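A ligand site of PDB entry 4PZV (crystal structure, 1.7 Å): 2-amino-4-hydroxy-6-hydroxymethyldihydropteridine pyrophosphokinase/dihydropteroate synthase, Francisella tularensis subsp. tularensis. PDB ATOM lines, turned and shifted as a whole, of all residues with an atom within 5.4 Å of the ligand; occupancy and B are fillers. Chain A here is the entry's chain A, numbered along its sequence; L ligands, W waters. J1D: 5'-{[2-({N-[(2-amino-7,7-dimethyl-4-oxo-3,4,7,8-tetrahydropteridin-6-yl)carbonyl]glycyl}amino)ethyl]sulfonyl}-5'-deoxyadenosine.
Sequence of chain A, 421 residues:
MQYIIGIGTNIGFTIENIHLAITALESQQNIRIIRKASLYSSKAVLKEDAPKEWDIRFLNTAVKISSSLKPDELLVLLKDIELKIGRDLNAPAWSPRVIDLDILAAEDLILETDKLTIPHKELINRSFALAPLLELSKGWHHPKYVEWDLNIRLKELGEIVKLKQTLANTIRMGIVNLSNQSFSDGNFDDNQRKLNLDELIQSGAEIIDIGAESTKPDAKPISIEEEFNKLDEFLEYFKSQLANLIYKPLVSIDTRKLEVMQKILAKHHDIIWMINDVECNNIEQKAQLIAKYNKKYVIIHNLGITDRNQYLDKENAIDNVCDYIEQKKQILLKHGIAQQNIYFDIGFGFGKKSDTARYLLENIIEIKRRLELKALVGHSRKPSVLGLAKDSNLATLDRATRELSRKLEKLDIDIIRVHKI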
ATOM      1  N   GLY A   8     -23.441   1.461  15.553  1.00  0.00           N
ATOM      2  CA  GLY A   8     -24.470   0.718  16.255  1.00  0.00           C
ATOM      3  C   GLY A   8     -25.675   0.497  15.361  1.00  0.00           C
ATOM      4  O   GLY A   8     -25.950   1.283  14.442  1.00  0.00           O
ATOM      5  N   SER A  42     -25.037  -6.146  22.975  1.00  0.00           N
ATOM      6  CA  SER A  42     -25.465  -5.632  24.269  1.00  0.00           C
ATOM      7  C   SER A  42     -26.940  -5.318  24.276  1.00  0.00           C
ATOM      8  O   SER A  42     -27.532  -5.085  23.226  1.00  0.00           O
ATOM      9  CB  SER A  42     -24.652  -4.383  24.673  1.00  0.00           C
ATOM     10  OG  SER A  42     -24.743  -3.368  23.667  1.00  0.00           O
ATOM     11  N   LYS A  43     -27.542  -5.311  25.460  1.00  0.00           N
ATOM     12  CA  LYS A  43     -28.913  -4.844  25.606  1.00  0.00           C
ATOM     13  C   LYS A  43     -29.009  -3.363  25.307  1.00  0.00           C
ATOM     14  O   LYS A  43     -28.145  -2.588  25.693  1.00  0.00           O
ATOM     15  CB  LYS A  43     -29.414  -5.066  27.020  1.00  0.00           C
ATOM     16  CG  LYS A  43     -29.533  -6.530  27.395  1.00  0.00           C
ATOM     17  CD  LYS A  43     -30.182  -6.643  28.750  1.00  0.00           C
ATOM     18  CE  LYS A  43     -30.331  -8.083  29.211  1.00  0.00           C
ATOM     19  NZ  LYS A  43     -31.080  -8.108  30.508  1.00  0.00           N
ATOM     20  N   ALA A  44     -30.082  -2.979  24.615  1.00  0.00           N
ATOM     21  CA  ALA A  44     -30.387  -1.585  24.401  1.00  0.00           C
ATOM     22  C   ALA A  44     -30.275  -0.853  25.732  1.00  0.00           C
ATOM     23  O   ALA A  44     -30.858  -1.274  26.714  1.00  0.00           O
ATOM     24  CB  ALA A  44     -31.802  -1.440  23.838  1.00  0.00           C
ATOM     25  N   VAL A  45     -29.490   0.199  25.752  1.00  0.00           N
ATOM     26  CA  VAL A  45     -29.466   1.118  26.888  1.00  0.00           C
ATOM     27  C   VAL A  45     -30.632   2.086  26.715  1.00  0.00           C
ATOM     28  O   VAL A  45     -30.664   2.868  25.759  1.00  0.00           O
ATOM     29  CB  VAL A  45     -28.155   1.885  26.941  1.00  0.00           C
ATOM     30  CG1 VAL A  45     -28.179   2.884  28.089  1.00  0.00           C
ATOM     31  CG2 VAL A  45     -26.990   0.911  27.106  1.00  0.00           C
ATOM     32  N   LEU A  46     -31.588   2.001  27.627  1.00  0.00           N
ATOM     33  CA  LEU A  46     -32.823   2.765  27.513  1.00  0.00           C
ATOM     34  C   LEU A  46     -33.091   3.565  28.765  1.00  0.00           C
ATOM     35  O   LEU A  46     -32.608   3.249  29.852  1.00  0.00           O
ATOM     36  CB  LEU A  46     -34.018   1.852  27.328  1.00  0.00           C
ATOM     37  CG  LEU A  46     -34.039   0.969  26.097  1.00  0.00           C
ATOM     38  CD1 LEU A  46     -35.366   0.265  25.978  1.00  0.00           C
ATOM     39  CD2 LEU A  46     -33.795   1.823  24.907  1.00  0.00           C
ATOM     40  N   PHE A  58     -28.554  -4.806  20.607  1.00  0.00           N
ATOM     41  CA  PHE A  58     -27.722  -4.027  19.687  1.00  0.00           C
ATOM     42  C   PHE A  58     -26.565  -4.844  19.153  1.00  0.00           C
ATOM     43  O   PHE A  58     -26.063  -5.751  19.823  1.00  0.00           O
ATOM     44  CB  PHE A  58     -27.167  -2.782  20.399  1.00  0.00           C
ATOM     45  CG  PHE A  58     -27.989  -1.528  20.187  1.00  0.00           C
ATOM     46  CD1 PHE A  58     -29.137  -1.308  20.927  1.00  0.00           C
ATOM     47  CD2 PHE A  58     -27.598  -0.593  19.249  1.00  0.00           C
ATOM     48  CE1 PHE A  58     -29.890  -0.152  20.717  1.00  0.00           C
ATOM     49  CE2 PHE A  58     -28.330   0.538  19.046  1.00  0.00           C
ATOM     50  CZ  PHE A  58     -29.468   0.771  19.775  1.00  0.00           C
ATOM     51  N   ASN A  60     -22.822  -3.660  17.920  1.00  0.00           N
ATOM     52  CA  ASN A  60     -21.947  -2.474  17.926  1.00  0.00           C
ATOM     53  C   ASN A  60     -20.532  -2.817  17.487  1.00  0.00           C
ATOM     54  O   ASN A  60     -20.073  -3.941  17.686  1.00  0.00           O
ATOM     55  CB  ASN A  60     -21.847  -1.840  19.328  1.00  0.00           C
ATOM     56  CG  ASN A  60     -23.085  -1.060  19.714  1.00  0.00           C
ATOM     57  OD1 ASN A  60     -23.987  -1.594  20.362  1.00  0.00           O
ATOM     58  ND2 ASN A  60     -23.124   0.211  19.368  1.00  0.00           N
ATOM     59  N   LEU A  75     -18.660  14.996  10.798  1.00  0.00           N
ATOM     60  CA  LEU A  75     -19.977  14.781  11.406  1.00  0.00           C
ATOM     61  C   LEU A  75     -21.063  14.889  10.344  1.00  0.00           C
ATOM     62  O   LEU A  75     -21.983  14.068  10.291  1.00  0.00           O
ATOM     63  CB  LEU A  75     -20.236  15.753  12.563  1.00  0.00           C
ATOM     64  CG  LEU A  75     -21.638  15.604  13.172  1.00  0.00           C
ATOM     65  CD1 LEU A  75     -21.770  14.254  13.871  1.00  0.00           C
ATOM     66  CD2 LEU A  75     -21.988  16.721  14.118  1.00  0.00           C
ATOM     67  N   LYS A  79     -23.818  11.867   9.253  1.00  0.00           N
ATOM     68  CA  LYS A  79     -25.257  12.050   9.145  1.00  0.00           C
ATOM     69  C   LYS A  79     -25.745  11.696   7.737  1.00  0.00           C
ATOM     70  O   LYS A  79     -26.765  11.018   7.566  1.00  0.00           O
ATOM     71  CB  LYS A  79     -25.634  13.502   9.452  1.00  0.00           C
ATOM     72  CG  LYS A  79     -25.218  13.983  10.836  1.00  0.00           C
ATOM     73  CD  LYS A  79     -25.719  15.388  11.071  1.00  0.00           C
ATOM     74  CE  LYS A  79     -25.286  15.905  12.423  1.00  0.00           C
ATOM     75  NZ  LYS A  79     -25.940  17.196  12.710  1.00  0.00           N
ATOM     76  N   ARG A  87     -31.872   5.846   8.132  1.00  0.00           N
ATOM     77  CA  ARG A  87     -32.252   6.231   9.481  1.00  0.00           C
ATOM     78  C   ARG A  87     -33.145   7.454   9.431  1.00  0.00           C
ATOM     79  O   ARG A  87     -32.963   8.302   8.579  1.00  0.00           O
ATOM     80  CB  ARG A  87     -31.003   6.550  10.314  1.00  0.00           C
ATOM     81  CG  ARG A  87     -31.348   6.878  11.750  1.00  0.00           C
ATOM     82  CD  ARG A  87     -30.164   7.238  12.591  1.00  0.00           C
ATOM     83  NE  ARG A  87     -30.603   7.420  13.972  1.00  0.00           N
ATOM     84  CZ  ARG A  87     -29.793   7.592  15.006  1.00  0.00           C
ATOM     85  NH1 ARG A  87     -28.478   7.598  14.854  1.00  0.00           N
ATOM     86  NH2 ARG A  87     -30.302   7.720  16.214  1.00  0.00           N
ATOM     87  N   TRP A  94     -33.461   7.440  21.790  1.00  0.00           N
ATOM     88  CA  TRP A  94     -33.517   6.130  22.425  1.00  0.00           C
ATOM     89  C   TRP A  94     -34.242   5.057  21.603  1.00  0.00           C
ATOM     90  O   TRP A  94     -34.192   3.872  21.967  1.00  0.00           O
ATOM     91  CB  TRP A  94     -34.163   6.237  23.803  1.00  0.00           C
ATOM     92  CG  TRP A  94     -33.603   7.334  24.666  1.00  0.00           C
ATOM     93  CD1 TRP A  94     -34.100   8.603  24.805  1.00  0.00           C
ATOM     94  CD2 TRP A  94     -32.446   7.258  25.499  1.00  0.00           C
ATOM     95  NE1 TRP A  94     -33.307   9.322  25.690  1.00  0.00           N
ATOM     96  CE2 TRP A  94     -32.285   8.516  26.127  1.00  0.00           C
ATOM     97  CE3 TRP A  94     -31.527   6.252  25.796  1.00  0.00           C
ATOM     98  CZ2 TRP A  94     -31.256   8.780  27.019  1.00  0.00           C
ATOM     99  CZ3 TRP A  94     -30.499   6.509  26.681  1.00  0.00           C
ATOM    100  CH2 TRP A  94     -30.372   7.771  27.282  1.00  0.00           C
ATOM    101  N   SER A  95     -34.916   5.444  20.531  1.00  0.00           N
ATOM    102  CA  SER A  95     -35.683   4.484  19.746  1.00  0.00           C
ATOM    103  C   SER A  95     -34.771   3.642  18.851  1.00  0.00           C
ATOM    104  O   SER A  95     -33.614   3.984  18.643  1.00  0.00           O
ATOM    105  CB  SER A  95     -36.758   5.182  18.917  1.00  0.00           C
ATOM    106  OG  SER A  95     -36.182   5.952  17.887  1.00  0.00           O
ATOM    107  N   ARG A  97     -32.938   1.910  15.629  1.00  0.00           N
ATOM    108  CA  ARG A  97     -32.374   2.603  14.467  1.00  0.00           C
ATOM    109  C   ARG A  97     -31.606   1.647  13.598  1.00  0.00           C
ATOM    110  O   ARG A  97     -30.941   0.736  14.091  1.00  0.00           O
ATOM    111  CB  ARG A  97     -31.452   3.751  14.887  1.00  0.00           C
ATOM    112  CG  ARG A  97     -30.085   3.325  15.441  1.00  0.00           C
ATOM    113  CD  ARG A  97     -30.184   2.762  16.875  1.00  0.00           C
ATOM    114  NE  ARG A  97     -30.923   3.686  17.717  1.00  0.00           N
ATOM    115  CZ  ARG A  97     -30.385   4.702  18.401  1.00  0.00           C
ATOM    116  NH1 ARG A  97     -29.074   4.905  18.396  1.00  0.00           N
ATOM    117  NH2 ARG A  97     -31.162   5.515  19.103  1.00  0.00           N
ATOM    118  N   ASP A 100     -26.325   3.945  13.333  1.00  0.00           N
ATOM    119  CA  ASP A 100     -25.980   5.092  14.151  1.00  0.00           C
ATOM    120  C   ASP A 100     -24.460   5.214  14.099  1.00  0.00           C
ATOM    121  O   ASP A 100     -23.749   4.228  14.325  1.00  0.00           O
ATOM    122  CB  ASP A 100     -26.511   4.882  15.569  1.00  0.00           C
ATOM    123  CG  ASP A 100     -25.689   5.595  16.629  1.00  0.00           C
ATOM    124  OD1 ASP A 100     -25.852   6.830  16.793  1.00  0.00           O
ATOM    125  OD2 ASP A 100     -24.884   4.910  17.289  1.00  0.00           O
ATOM    126  N   LEU A 101     -23.975   6.401  13.732  1.00  0.00           N
ATOM    127  CA  LEU A 101     -22.540   6.641  13.583  1.00  0.00           C
ATOM    128  C   LEU A 101     -22.149   7.862  14.402  1.00  0.00           C
ATOM    129  O   LEU A 101     -22.748   8.928  14.260  1.00  0.00           O
ATOM    130  CB  LEU A 101     -22.207   6.893  12.126  1.00  0.00           C
ATOM    131  CG  LEU A 101     -22.664   5.787  11.186  1.00  0.00           C
ATOM    132  CD1 LEU A 101     -22.378   6.145   9.773  1.00  0.00           C
ATOM    133  CD2 LEU A 101     -21.929   4.533  11.548  1.00  0.00           C
ATOM    134  N   ASP A 102     -21.146   7.710  15.242  1.00  0.00           N
ATOM    135  CA  ASP A 102     -20.667   8.855  16.002  1.00  0.00           C
ATOM    136  C   ASP A 102     -19.154   8.878  16.075  1.00  0.00           C
ATOM    137  O   ASP A 102     -18.488   7.884  15.783  1.00  0.00           O
ATOM    138  CB  ASP A 102     -21.267   8.855  17.403  1.00  0.00           C
ATOM    139  CG  ASP A 102     -21.192   7.507  18.076  1.00  0.00           C
ATOM    140  OD1 ASP A 102     -20.221   6.774  17.822  1.00  0.00           O
ATOM    141  OD2 ASP A 102     -22.120   7.176  18.842  1.00  0.00           O
ATOM    142  N   ILE A 103     -18.621  10.035  16.427  1.00  0.00           N
ATOM    143  CA  ILE A 103     -17.189  10.202  16.591  1.00  0.00           C
ATOM    144  C   ILE A 103     -16.878   9.920  18.053  1.00  0.00           C
ATOM    145  O   ILE A 103     -17.226  10.732  18.918  1.00  0.00           O
ATOM    146  CB  ILE A 103     -16.681  11.591  16.194  1.00  0.00           C
ATOM    147  CG1 ILE A 103     -17.143  11.960  14.785  1.00  0.00           C
ATOM    148  CG2 ILE A 103     -15.164  11.617  16.290  1.00  0.00           C
ATOM    149  CD1 ILE A 103     -16.850  13.415  14.396  1.00  0.00           C
ATOM    150  N   LEU A 104     -16.255   8.785  18.331  1.00  0.00           N
ATOM    151  CA  LEU A 104     -15.934   8.434  19.706  1.00  0.00           C
ATOM    152  C   LEU A 104     -14.703   9.166  20.241  1.00  0.00           C
ATOM    153  O   LEU A 104     -14.669   9.593  21.388  1.00  0.00           O
ATOM    154  CB  LEU A 104     -15.681   6.929  19.820  1.00  0.00           C
ATOM    155  CG  LEU A 104     -16.875   6.016  19.531  1.00  0.00           C
ATOM    156  CD1 LEU A 104     -16.501   4.595  19.843  1.00  0.00           C
ATOM    157  CD2 LEU A 104     -18.100   6.414  20.334  1.00  0.00           C
ATOM    158  N   ASP A 114     -21.875  22.638  21.470  1.00  0.00           N
ATOM    159  CA  ASP A 114     -23.223  22.127  21.635  1.00  0.00           C
ATOM    160  C   ASP A 114     -23.506  21.054  20.606  1.00  0.00           C
ATOM    161  O   ASP A 114     -24.199  20.081  20.894  1.00  0.00           O
ATOM    162  CB  ASP A 114     -24.252  23.245  21.472  1.00  0.00           C
ATOM    163  CG  ASP A 114     -24.281  24.187  22.656  1.00  0.00           C
ATOM    164  OD1 ASP A 114     -23.500  25.177  22.638  1.00  0.00           O
ATOM    165  OD2 ASP A 114     -25.049  23.917  23.611  1.00  0.00           O
ATOM    166  N   LYS A 115     -22.993  21.240  19.406  1.00  0.00           N
ATOM    167  CA  LYS A 115     -23.323  20.376  18.293  1.00  0.00           C
ATOM    168  C   LYS A 115     -22.436  19.123  18.250  1.00  0.00           C
ATOM    169  O   LYS A 115     -22.830  18.070  17.736  1.00  0.00           O
ATOM    170  CB  LYS A 115     -23.177  21.163  16.994  1.00  0.00           C
ATOM    171  CG  LYS A 115     -23.684  20.448  15.790  1.00  0.00           C
ATOM    172  CD  LYS A 115     -23.319  21.172  14.507  1.00  0.00           C
ATOM    173  CE  LYS A 115     -21.818  21.182  14.262  1.00  0.00           C
ATOM    174  NZ  LYS A 115     -21.513  21.675  12.877  1.00  0.00           N
ATOM    175  N   LEU A 116     -21.235  19.248  18.791  1.00  0.00           N
ATOM    176  CA  LEU A 116     -20.250  18.165  18.730  1.00  0.00           C
ATOM    177  C   LEU A 116     -19.337  18.182  19.957  1.00  0.00           C
ATOM    178  O   LEU A 116     -18.745  19.208  20.300  1.00  0.00           O
ATOM    179  CB  LEU A 116     -19.449  18.276  17.435  1.00  0.00           C
ATOM    180  CG  LEU A 116     -18.356  17.247  17.164  1.00  0.00           C
ATOM    181  CD1 LEU A 116     -18.856  15.808  17.340  1.00  0.00           C
ATOM    182  CD2 LEU A 116     -17.767  17.452  15.773  1.00  0.00           C
ATOM    183  N   THR A 117     -19.265  17.042  20.651  1.00  0.00           N
ATOM    184  CA  THR A 117     -18.358  16.898  21.779  1.00  0.00           C
ATOM    185  C   THR A 117     -17.490  15.670  21.558  1.00  0.00           C
ATOM    186  O   THR A 117     -18.007  14.572  21.338  1.00  0.00           O
ATOM    187  CB  THR A 117     -19.121  16.749  23.117  1.00  0.00           C
ATOM    188  OG1 THR A 117     -19.930  17.926  23.366  1.00  0.00           O
ATOM    189  CG2 THR A 117     -18.133  16.552  24.273  1.00  0.00           C
ATOM    190  N   ILE A 118     -16.176  15.867  21.637  1.00  0.00           N
ATOM    191  CA  ILE A 118     -15.206  14.802  21.443  1.00  0.00           C
ATOM    192  C   ILE A 118     -14.163  14.859  22.550  1.00  0.00           C
ATOM    193  O   ILE A 118     -13.627  15.930  22.844  1.00  0.00           O
ATOM    194  CB  ILE A 118     -14.482  14.960  20.099  1.00  0.00           C
ATOM    195  CG1 ILE A 118     -15.483  14.990  18.953  1.00  0.00           C
ATOM    196  CG2 ILE A 118     -13.426  13.858  19.905  1.00  0.00           C
ATOM    197  CD1 ILE A 118     -14.885  15.391  17.633  1.00  0.00           C
ATOM    198  N   PRO A 119     -13.867  13.710  23.186  1.00  0.00           N
ATOM    199  CA  PRO A 119     -14.537  12.421  22.914  1.00  0.00           C
ATOM    200  C   PRO A 119     -16.022  12.505  23.210  1.00  0.00           C
ATOM    201  O   PRO A 119     -16.483  13.412  23.894  1.00  0.00           O
ATOM    202  CB  PRO A 119     -13.840  11.460  23.883  1.00  0.00           C
ATOM    203  CG  PRO A 119     -12.552  12.137  24.250  1.00  0.00           C
ATOM    204  CD  PRO A 119     -12.832  13.596  24.217  1.00  0.00           C
ATOM    205  N   HIS A 120     -16.776  11.562  22.646  1.00  0.00           N
ATOM    206  CA  HIS A 120     -18.203  11.504  22.850  1.00  0.00           C
ATOM    207  C   HIS A 120     -18.494  11.462  24.335  1.00  0.00           C
ATOM    208  O   HIS A 120     -17.815  10.778  25.095  1.00  0.00           O
ATOM    209  CB  HIS A 120     -18.767  10.262  22.203  1.00  0.00           C
ATOM    210  CG  HIS A 120     -20.249  10.223  22.156  1.00  0.00           C
ATOM    211  ND1 HIS A 120     -21.029   9.998  23.271  1.00  0.00           N
ATOM    212  CD2 HIS A 120     -21.117  10.369  21.116  1.00  0.00           C
ATOM    213  CE1 HIS A 120     -22.312  10.018  22.926  1.00  0.00           C
ATOM    214  NE2 HIS A 120     -22.387  10.233  21.628  1.00  0.00           N
ATOM    215  N   ARG A 126     -20.204   3.821  28.397  1.00  0.00           N
ATOM    216  CA  ARG A 126     -20.830   2.860  27.474  1.00  0.00           C
ATOM    217  C   ARG A 126     -19.850   1.777  26.992  1.00  0.00           C
ATOM    218  O   ARG A 126     -18.941   2.033  26.212  1.00  0.00           O
ATOM    219  CB  ARG A 126     -21.468   3.611  26.287  1.00  0.00           C
ATOM    220  CG  ARG A 126     -22.716   4.378  26.684  1.00  0.00           C
ATOM    221  CD  ARG A 126     -23.275   5.318  25.622  1.00  0.00           C
ATOM    222  NE  ARG A 126     -24.522   5.926  26.102  1.00  0.00           N
ATOM    223  CZ  ARG A 126     -25.194   6.911  25.494  1.00  0.00           C
ATOM    224  NH1 ARG A 126     -24.764   7.433  24.354  1.00  0.00           N
ATOM    225  NH2 ARG A 126     -26.313   7.377  26.049  1.00  0.00           N
ATOM    226  N   PHE A 128     -20.310  -0.686  25.000  1.00  0.00           N
ATOM    227  CA  PHE A 128     -20.412  -1.038  23.582  1.00  0.00           C
ATOM    228  C   PHE A 128     -19.626  -0.083  22.699  1.00  0.00           C
ATOM    229  O   PHE A 128     -19.381  -0.382  21.520  1.00  0.00           O
ATOM    230  CB  PHE A 128     -21.870  -1.113  23.117  1.00  0.00           C
ATOM    231  CG  PHE A 128     -22.674   0.094  23.458  1.00  0.00           C
ATOM    232  CD1 PHE A 128     -22.607   1.220  22.677  1.00  0.00           C
ATOM    233  CD2 PHE A 128     -23.519   0.091  24.558  1.00  0.00           C
ATOM    234  CE1 PHE A 128     -23.339   2.356  22.983  1.00  0.00           C
ATOM    235  CE2 PHE A 128     -24.273   1.228  24.863  1.00  0.00           C
ATOM    236  CZ  PHE A 128     -24.176   2.342  24.078  1.00  0.00           C
HETATM  237  C1  J1D L   1     -26.401  14.320  17.585  1.00  0.00           C
HETATM  238  O1  J1D L   1     -25.405  14.339  18.609  1.00  0.00           O
HETATM  239  C2  J1D L   1     -25.654  14.746  16.301  1.00  0.00           C
HETATM  240  O2  J1D L   1     -26.560  15.444  15.515  1.00  0.00           O
HETATM  241  C3  J1D L   1     -24.542  15.683  16.824  1.00  0.00           C
HETATM  242  O3  J1D L   1     -24.970  16.997  16.725  1.00  0.00           O
HETATM  243  C4  J1D L   1     -24.498  15.372  18.350  1.00  0.00           C
HETATM  244  N1  J1D L   1     -23.161  14.942  18.753  1.00  0.00           N
HETATM  245  C5  J1D L   1     -22.357  15.466  19.776  1.00  0.00           C
HETATM  246  N2  J1D L   1     -21.197  14.848  19.901  1.00  0.00           N
HETATM  247  C6  J1D L   1     -21.213  13.882  18.911  1.00  0.00           C
HETATM  248  C7  J1D L   1     -20.293  12.918  18.528  1.00  0.00           C
HETATM  249  N3  J1D L   1     -19.099  12.824  19.164  1.00  0.00           N
HETATM  250  N4  J1D L   1     -20.605  12.057  17.503  1.00  0.00           N
HETATM  251  C8  J1D L   1     -21.799  12.217  16.889  1.00  0.00           C
HETATM  252  N5  J1D L   1     -22.787  13.089  17.144  1.00  0.00           N
HETATM  253  C9  J1D L   1     -22.446  13.914  18.172  1.00  0.00           C
HETATM  254  C10 J1D L   1     -26.988  12.948  17.432  1.00  0.00           C
HETATM  255  S1  J1D L   1     -27.909  12.486  18.836  1.00  0.00           S
HETATM  256  C11 J1D L   1     -28.777  11.305  18.547  1.00  0.00           C
HETATM  257  N6  J1D L   1     -27.361   9.493  18.928  1.00  0.00           N
HETATM  258  C12 J1D L   1     -28.199  10.164  17.912  1.00  0.00           C
HETATM  259  C13 J1D L   1     -27.515   8.162  19.283  1.00  0.00           C
HETATM  260  C14 J1D L   1     -26.499   7.774  20.337  1.00  0.00           C
HETATM  261  N7  J1D L   1     -26.700   6.434  20.848  1.00  0.00           N
HETATM  262  C15 J1D L   1     -27.863   6.053  21.458  1.00  0.00           C
HETATM  263  O4  J1D L   1     -28.833   6.798  21.622  1.00  0.00           O
HETATM  264  N8  J1D L   1     -27.684   0.827  23.516  1.00  0.00           N
HETATM  265  C16 J1D L   1     -26.718   0.030  22.961  1.00  0.00           C
HETATM  266  N9  J1D L   1     -26.533  -1.238  23.455  1.00  0.00           N
HETATM  267  N10 J1D L   1     -25.877   0.373  21.926  1.00  0.00           N
HETATM  268  C17 J1D L   1     -25.995   1.638  21.366  1.00  0.00           C
HETATM  269  O5  J1D L   1     -25.179   1.932  20.375  1.00  0.00           O
HETATM  270  N11 J1D L   1     -27.081   3.783  21.315  1.00  0.00           N
HETATM  271  C18 J1D L   1     -27.882   4.627  21.926  1.00  0.00           C
HETATM  272  C19 J1D L   1     -28.929   4.283  22.920  1.00  0.00           C
HETATM  273  C20 J1D L   1     -30.280   4.366  22.222  1.00  0.00           C
HETATM  274  C21 J1D L   1     -28.828   5.215  24.119  1.00  0.00           C
HETATM  275  N12 J1D L   1     -28.742   2.911  23.437  1.00  0.00           N
HETATM  276  C22 J1D L   1     -27.799   2.068  22.949  1.00  0.00           C
HETATM  277  C23 J1D L   1     -26.971   2.523  21.872  1.00  0.00           C
HETATM  278  O6  J1D L   1     -28.358   7.408  18.800  1.00  0.00           O
HETATM  279  O7  J1D L   1     -28.595  13.604  19.785  1.00  0.00           O
HETATM  280  O8  J1D L   1     -26.745  12.051  19.896  1.00  0.00           O
HETATM  281  O   HOH W   1     -24.933   9.940  16.458  1.00  0.00           O
HETATM  282  O   HOH W   2     -22.376  17.918  22.067  1.00  0.00           O
HETATM  283  O   HOH W   3     -28.545  13.606  14.096  1.00  0.00           O
HETATM  284  O   HOH W   4     -24.520  11.016  19.926  1.00  0.00           O
HETATM  285  O   HOH W   5     -25.839  10.233  22.480  1.00  0.00           O
HETATM  286  O   HOH W   6     -25.808  17.541  20.383  1.00  0.00           O
HETATM  287  O   HOH W   7     -20.993  13.518  22.698  1.00  0.00           O
HETATM  288  O   HOH W   8     -31.704   8.014  20.195  1.00  0.00           O
HETATM  289  O   HOH W   9     -26.468   2.841  18.073  1.00  0.00           O
HETATM  290  O   HOH W  10     -25.804  18.407  14.788  1.00  0.00           O
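Water W4 lies within hydrogen-bond range of O8 of the ligand and NE2 of His 120.
Water W10 bridges NZ of Lys 79 (2.4 Å) and O3 of the ligand (2.5 Å).
Water W9 lies within hydrogen-bond range of the side-chain carboxylate of Asp 100 (2.7 Å), an oxygen (O5) of the ligand (2.8 Å) and the guanidinium group of Arg 97 (3.3 Å).
Water W7 bridges a nitrogen (N2) of the ligand (3.1 Å) and the backbone carbonyl oxygen of Thr 117 (3.4 Å).
Water W8 lies within hydrogen-bond range of the backbone NH (N) of Trp 94 (2.4 Å), the guanidinium group (NH2) of Arg 97 (2.8 Å) and an oxygen (O4) of the ligand (3.4 Å).
Water W1 lies within hydrogen-bond range of OD1 of Asp 100 (3.3 Å), O of Leu 101 (3.3 Å) and N6 of the ligand (3.5 Å).
The backbone carbonyl oxygen (O) of Lys 115 lies within hydrogen-bond range of an oxygen (O3) of the ligand, at 2.6 Å.
O6 of the ligand sits at hydrogen-bond distance from NH1 of Arg 97, at 2.6 Å.
The side-chain hydroxyl of Ser 42 lies within hydrogen-bond range of a nitrogen (N9) of the ligand (2.8 Å).
The backbone NH (N) of Ile 103 is in hydrogen-bond range of a nitrogen (N4) of the ligand.
N3 of the ligand sits at hydrogen-bond distance from O of Ile 103 (2.8 Å).
The side-chain amide nitrogen (ND2) of Asn 60 is in hydrogen-bond range of an oxygen (O5) of the ligand.
The backbone NH (N) of Val 45 is in hydrogen-bond range of a nitrogen (N8) of the ligand (2.9 Å).
The backbone carbonyl oxygen (O) of Val 45 sits at hydrogen-bond distance from a nitrogen (N12) of the ligand, 3.0 Å away.
A nitrogen (N2) of the ligand lies within hydrogen-bond range of the backbone NH (N) of Thr 117 (3.0 Å).
The backbone carbonyl oxygen (O) of Thr 117 is in hydrogen-bond range of a nitrogen (N3) of the ligand (3.0 Å).
A nitrogen (N9) of the ligand sits at hydrogen-bond distance from the backbone carbonyl oxygen of Lys 43, at 3.1 Å.
The guanidinium group (NH2) of Arg 87 lies within hydrogen-bond range of an oxygen (O6) of the ligand, 3.3 Å away.
NZ of Lys 79 sits at hydrogen-bond distance from O2 of the ligand (3.4 Å).
The side-chain carboxylate of Asp 100 sits close to an oxygen (O6) of the ligand, 3.3 Å away.
CA of Ala 44 touches N8 of the ligand (3.7 Å).
Phe 58 touches the ligand (CD2 to N10, 3.3 Å).
CD1 of Leu 75 touches N5 of the ligand, 3.6 Å away.
Trp 94 touches the ligand (CZ3 to C21, 3.3 Å).
Asp 102 touches the ligand.
Leu 116 touches the ligand.
His 120 touches the ligand (CD2 to C7, 3.7 Å).
Arg 126 touches the ligand.
Phe 128 touches the ligand (CE1 to C17, 3.2 Å).
Hydrophobic or aromatic side chains that line the ligand: Val 45, Phe 58, Leu 75, Trp 94, Leu 116, His 120 and Phe 128.
Along chain A the residues within 4 Å of the ligand span positions 42 to 128.
The nearest printed residue that does not touch the ligand is Ile 118 (4.2 Å).
O of Ser 95 sits at hydrogen-bond distance from NE of Arg 97 (2.9 Å).
The backbone NH (N) of Phe 58 is in hydrogen-bond range of the backbone carbonyl oxygen (O) of Ser 42 (2.8 Å).
The guanidinium group (NH1) of Arg 87 lies within salt-bridge range of the side-chain carboxylate (OD1) of Asp 100.
N of Asp 100 sits at hydrogen-bond distance from O of Gly 8 (2.9 Å).
O of Leu 104 is in hydrogen-bond range of N of His 120.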
